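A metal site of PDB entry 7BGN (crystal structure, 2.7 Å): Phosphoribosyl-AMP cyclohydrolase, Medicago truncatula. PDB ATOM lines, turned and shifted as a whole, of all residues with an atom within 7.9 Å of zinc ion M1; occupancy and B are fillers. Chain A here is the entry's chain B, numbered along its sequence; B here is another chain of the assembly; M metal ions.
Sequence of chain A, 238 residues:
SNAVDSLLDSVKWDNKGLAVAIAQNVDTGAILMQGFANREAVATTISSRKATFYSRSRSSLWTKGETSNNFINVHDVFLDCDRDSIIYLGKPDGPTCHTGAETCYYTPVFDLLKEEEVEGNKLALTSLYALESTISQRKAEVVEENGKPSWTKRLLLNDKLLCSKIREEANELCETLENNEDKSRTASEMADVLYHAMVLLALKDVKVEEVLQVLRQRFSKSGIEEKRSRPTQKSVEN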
ATOM      1  N   LEU A  32     -16.507 -10.209  -1.618  1.00  0.00           N
ATOM      2  CA  LEU A  32     -17.291 -11.208  -0.894  1.00  0.00           C
ATOM      3  C   LEU A  32     -18.778 -10.912  -0.941  1.00  0.00           C
ATOM      4  O   LEU A  32     -19.593 -11.791  -1.248  1.00  0.00           O
ATOM      5  CB  LEU A  32     -16.822 -11.290   0.559  1.00  0.00           C
ATOM      6  CG  LEU A  32     -15.333 -11.574   0.730  1.00  0.00           C
ATOM      7  CD1 LEU A  32     -14.967 -11.677   2.196  1.00  0.00           C
ATOM      8  CD2 LEU A  32     -14.929 -12.826  -0.047  1.00  0.00           C
ATOM      9  N   MET A  33     -19.153  -9.666  -0.652  1.00  0.00           N
ATOM     10  CA  MET A  33     -20.546  -9.271  -0.509  1.00  0.00           C
ATOM     11  C   MET A  33     -20.589  -7.762  -0.446  1.00  0.00           C
ATOM     12  O   MET A  33     -19.577  -7.100  -0.190  1.00  0.00           O
ATOM     13  CB  MET A  33     -21.175  -9.872   0.756  1.00  0.00           C
ATOM     14  CG  MET A  33     -20.428  -9.488   2.036  1.00  0.00           C
ATOM     15  SD  MET A  33     -21.402  -9.544   3.559  1.00  0.00           S
ATOM     16  CE  MET A  33     -22.616  -8.261   3.251  1.00  0.00           C
ATOM     17  N   TRP A  62     -26.089  -6.045  12.084  1.00  0.00           N
ATOM     18  CA  TRP A  62     -25.855  -7.427  11.671  1.00  0.00           C
ATOM     19  C   TRP A  62     -24.378  -7.620  11.373  1.00  0.00           C
ATOM     20  O   TRP A  62     -23.832  -6.971  10.468  1.00  0.00           O
ATOM     21  CB  TRP A  62     -26.716  -7.770  10.442  1.00  0.00           C
ATOM     22  CG  TRP A  62     -26.197  -8.940   9.641  1.00  0.00           C
ATOM     23  CD1 TRP A  62     -25.990 -10.216  10.091  1.00  0.00           C
ATOM     24  CD2 TRP A  62     -25.856  -8.945   8.251  1.00  0.00           C
ATOM     25  NE1 TRP A  62     -25.521 -11.004   9.063  1.00  0.00           N
ATOM     26  CE2 TRP A  62     -25.426 -10.248   7.924  1.00  0.00           C
ATOM     27  CE3 TRP A  62     -25.856  -7.963   7.255  1.00  0.00           C
ATOM     28  CZ2 TRP A  62     -25.012 -10.603   6.644  1.00  0.00           C
ATOM     29  CZ3 TRP A  62     -25.444  -8.319   5.992  1.00  0.00           C
ATOM     30  CH2 TRP A  62     -25.024  -9.618   5.693  1.00  0.00           C
ATOM     31  N   LYS A  64     -21.715 -10.005   9.796  1.00  0.00           N
ATOM     32  CA  LYS A  64     -21.622 -11.152   8.900  1.00  0.00           C
ATOM     33  C   LYS A  64     -20.965 -12.318   9.609  1.00  0.00           C
ATOM     34  O   LYS A  64     -19.814 -12.210  10.057  1.00  0.00           O
ATOM     35  CB  LYS A  64     -20.843 -10.775   7.646  1.00  0.00           C
ATOM     36  CG  LYS A  64     -20.668 -11.921   6.686  1.00  0.00           C
ATOM     37  CD  LYS A  64     -21.989 -12.606   6.425  1.00  0.00           C
ATOM     38  CE  LYS A  64     -21.769 -13.994   5.870  1.00  0.00           C
ATOM     39  NZ  LYS A  64     -23.041 -14.685   5.499  1.00  0.00           N
ATOM     40  N   THR A  96     -18.978 -16.949   2.044  1.00  0.00           N
ATOM     41  CA  THR A  96     -19.651 -15.743   2.498  1.00  0.00           C
ATOM     42  C   THR A  96     -21.147 -15.794   2.221  1.00  0.00           C
ATOM     43  O   THR A  96     -21.947 -15.463   3.100  1.00  0.00           O
ATOM     44  CB  THR A  96     -19.017 -14.502   1.863  1.00  0.00           C
ATOM     45  OG1 THR A  96     -17.630 -14.446   2.200  1.00  0.00           O
ATOM     46  CG2 THR A  96     -19.706 -13.229   2.366  1.00  0.00           C
ATOM     47  N   CYS A  97     -21.549 -16.274   1.043  1.00  0.00           N
ATOM     48  CA  CYS A  97     -22.960 -16.263   0.694  1.00  0.00           C
ATOM     49  C   CYS A  97     -23.730 -17.311   1.487  1.00  0.00           C
ATOM     50  O   CYS A  97     -23.197 -18.360   1.860  1.00  0.00           O
ATOM     51  CB  CYS A  97     -23.174 -16.500  -0.797  1.00  0.00           C
ATOM     52  SG  CYS A  97     -24.945 -16.470  -1.295  1.00  0.00           S
ATOM     53  N   HIS A  98     -25.008 -17.013   1.734  1.00  0.00           N
ATOM     54  CA  HIS A  98     -25.843 -17.896   2.535  1.00  0.00           C
ATOM     55  C   HIS A  98     -26.176 -19.213   1.823  1.00  0.00           C
ATOM     56  O   HIS A  98     -26.564 -20.171   2.484  1.00  0.00           O
ATOM     57  CB  HIS A  98     -27.122 -17.150   2.958  1.00  0.00           C
ATOM     58  CG  HIS A  98     -28.274 -17.323   2.020  1.00  0.00           C
ATOM     59  ND1 HIS A  98     -28.417 -16.578   0.864  1.00  0.00           N
ATOM     60  CD2 HIS A  98     -29.375 -18.107   2.088  1.00  0.00           C
ATOM     61  CE1 HIS A  98     -29.539 -16.922   0.252  1.00  0.00           C
ATOM     62  NE2 HIS A  98     -30.134 -17.849   0.980  1.00  0.00           N
ATOM     63  N   THR A  99     -26.028 -19.272   0.501  1.00  0.00           N
ATOM     64  CA  THR A  99     -26.243 -20.505  -0.253  1.00  0.00           C
ATOM     65  C   THR A  99     -25.093 -21.492  -0.132  1.00  0.00           C
ATOM     66  O   THR A  99     -25.247 -22.647  -0.545  1.00  0.00           O
ATOM     67  CB  THR A  99     -26.465 -20.217  -1.744  1.00  0.00           C
ATOM     68  OG1 THR A  99     -25.241 -19.751  -2.331  1.00  0.00           O
ATOM     69  CG2 THR A  99     -27.516 -19.143  -1.937  1.00  0.00           C
ATOM     70  N   GLY A 100     -23.939 -21.063   0.361  1.00  0.00           N
ATOM     71  CA  GLY A 100     -22.755 -21.879   0.417  1.00  0.00           C
ATOM     72  C   GLY A 100     -21.700 -21.488  -0.586  1.00  0.00           C
ATOM     73  O   GLY A 100     -20.577 -22.019  -0.520  1.00  0.00           O
ATOM     74  N   ALA A 101     -21.995 -20.571  -1.494  1.00  0.00           N
ATOM     75  CA  ALA A 101     -21.011 -20.134  -2.474  1.00  0.00           C
ATOM     76  C   ALA A 101     -19.897 -19.363  -1.781  1.00  0.00           C
ATOM     77  O   ALA A 101     -20.099 -18.725  -0.743  1.00  0.00           O
ATOM     78  CB  ALA A 101     -21.677 -19.296  -3.558  1.00  0.00           C
ATOM     79  N   THR A 103     -18.267 -16.651  -2.651  1.00  0.00           N
ATOM     80  CA  THR A 103     -18.759 -15.275  -2.609  1.00  0.00           C
ATOM     81  C   THR A 103     -20.214 -15.244  -3.032  1.00  0.00           C
ATOM     82  O   THR A 103     -20.785 -16.253  -3.453  1.00  0.00           O
ATOM     83  CB  THR A 103     -17.915 -14.350  -3.505  1.00  0.00           C
ATOM     84  OG1 THR A 103     -18.177 -14.655  -4.879  1.00  0.00           O
ATOM     85  CG2 THR A 103     -16.462 -14.560  -3.229  1.00  0.00           C
ATOM     86  N   CYS A 104     -20.834 -14.065  -2.940  1.00  0.00           N
ATOM     87  CA  CYS A 104     -22.233 -13.911  -3.300  1.00  0.00           C
ATOM     88  C   CYS A 104     -22.444 -13.687  -4.783  1.00  0.00           C
ATOM     89  O   CYS A 104     -23.589 -13.734  -5.255  1.00  0.00           O
ATOM     90  CB  CYS A 104     -22.870 -12.735  -2.544  1.00  0.00           C
ATOM     91  SG  CYS A 104     -23.347 -13.017  -0.832  1.00  0.00           S
ATOM     92  N   TYR A 105     -21.387 -13.449  -5.550  1.00  0.00           N
ATOM     93  CA  TYR A 105     -21.512 -13.036  -6.942  1.00  0.00           C
ATOM     94  C   TYR A 105     -21.233 -14.229  -7.838  1.00  0.00           C
ATOM     95  O   TYR A 105     -20.072 -14.543  -8.120  1.00  0.00           O
ATOM     96  CB  TYR A 105     -20.588 -11.861  -7.207  1.00  0.00           C
ATOM     97  CG  TYR A 105     -20.957 -10.630  -6.398  1.00  0.00           C
ATOM     98  CD1 TYR A 105     -20.470 -10.439  -5.122  1.00  0.00           C
ATOM     99  CD2 TYR A 105     -21.812  -9.669  -6.927  1.00  0.00           C
ATOM    100  CE1 TYR A 105     -20.802  -9.320  -4.390  1.00  0.00           C
ATOM    101  CE2 TYR A 105     -22.149  -8.544  -6.202  1.00  0.00           C
ATOM    102  CZ  TYR A 105     -21.653  -8.379  -4.944  1.00  0.00           C
ATOM    103  OH  TYR A 105     -22.002  -7.257  -4.244  1.00  0.00           O
ATOM    104  N   TYR A 106     -22.297 -14.884  -8.306  1.00  0.00           N
ATOM    105  CA  TYR A 106     -22.116 -16.046  -9.173  1.00  0.00           C
ATOM    106  C   TYR A 106     -23.226 -16.161 -10.200  1.00  0.00           C
ATOM    107  O   TYR A 106     -23.528 -17.259 -10.664  1.00  0.00           O
ATOM    108  CB  TYR A 106     -22.074 -17.355  -8.363  1.00  0.00           C
ATOM    109  CG  TYR A 106     -23.231 -17.472  -7.409  1.00  0.00           C
ATOM    110  CD1 TYR A 106     -24.466 -17.954  -7.842  1.00  0.00           C
ATOM    111  CD2 TYR A 106     -23.091 -17.096  -6.077  1.00  0.00           C
ATOM    112  CE1 TYR A 106     -25.533 -18.051  -6.973  1.00  0.00           C
ATOM    113  CE2 TYR A 106     -24.152 -17.192  -5.195  1.00  0.00           C
ATOM    114  CZ  TYR A 106     -25.368 -17.668  -5.654  1.00  0.00           C
ATOM    115  OH  TYR A 106     -26.430 -17.772  -4.779  1.00  0.00           O
ATOM    116  N   ASP B  80     -25.489 -10.437  -7.644  1.00  0.00           N
ATOM    117  CA  ASP B  80     -25.372 -11.256  -6.444  1.00  0.00           C
ATOM    118  C   ASP B  80     -26.656 -12.084  -6.259  1.00  0.00           C
ATOM    119  O   ASP B  80     -27.551 -12.090  -7.102  1.00  0.00           O
ATOM    120  CB  ASP B  80     -25.053 -10.390  -5.216  1.00  0.00           C
ATOM    121  CG  ASP B  80     -26.151  -9.433  -4.869  1.00  0.00           C
ATOM    122  OD1 ASP B  80     -26.870  -8.995  -5.778  1.00  0.00           O
ATOM    123  OD2 ASP B  80     -26.297  -9.099  -3.662  1.00  0.00           O
ATOM    124  N   CYS B  81     -26.709 -12.807  -5.136  1.00  0.00           N
ATOM    125  CA  CYS B  81     -27.767 -13.789  -4.912  1.00  0.00           C
ATOM    126  C   CYS B  81     -29.158 -13.164  -4.864  1.00  0.00           C
ATOM    127  O   CYS B  81     -30.093 -13.662  -5.489  1.00  0.00           O
ATOM    128  CB  CYS B  81     -27.463 -14.568  -3.642  1.00  0.00           C
ATOM    129  SG  CYS B  81     -26.835 -13.551  -2.294  1.00  0.00           S
ATOM    130  N   ASP B  82     -29.316 -12.088  -4.087  1.00  0.00           N
ATOM    131  CA  ASP B  82     -30.582 -11.365  -3.991  1.00  0.00           C
ATOM    132  C   ASP B  82     -30.811 -10.415  -5.180  1.00  0.00           C
ATOM    133  O   ASP B  82     -31.880  -9.803  -5.256  1.00  0.00           O
ATOM    134  CB  ASP B  82     -30.636 -10.579  -2.676  1.00  0.00           C
ATOM    135  CG  ASP B  82     -29.353  -9.809  -2.397  1.00  0.00           C
ATOM    136  OD1 ASP B  82     -28.446  -9.834  -3.262  1.00  0.00           O
ATOM    137  OD2 ASP B  82     -29.249  -9.178  -1.332  1.00  0.00           O
HETATM  138 ZN    ZN M   1     -25.450 -14.305  -0.621  1.00  0.00          ZN
HETATM  139 ZN    ZN M   2     -27.562  -8.359  -2.226  1.00  0.00          ZN
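OG1 of Thr 99 sits close to SG of Cys 97 (3.5 Å).
The backbone carbonyl oxygen (O) of Leu 32 sits at hydrogen-bond distance from the backbone NH (N) of Cys 104 (3.1 Å).
N of His 98 touches zinc ion M1 (3.6 Å).
Of the 17 residues printed, 4 come within 4 Å of zinc ion M1.
The nearest printed residue that does not touch zinc ion M1 is Thr 99 (5.1 Å).
Zinc ion M1 is bound by the side-chain sulfur of Cys 81 of chain B (2.3 Å), the side-chain sulfur of Cys 97 (2.3 Å) and the side-chain sulfur of Cys 104 (2.5 Å).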
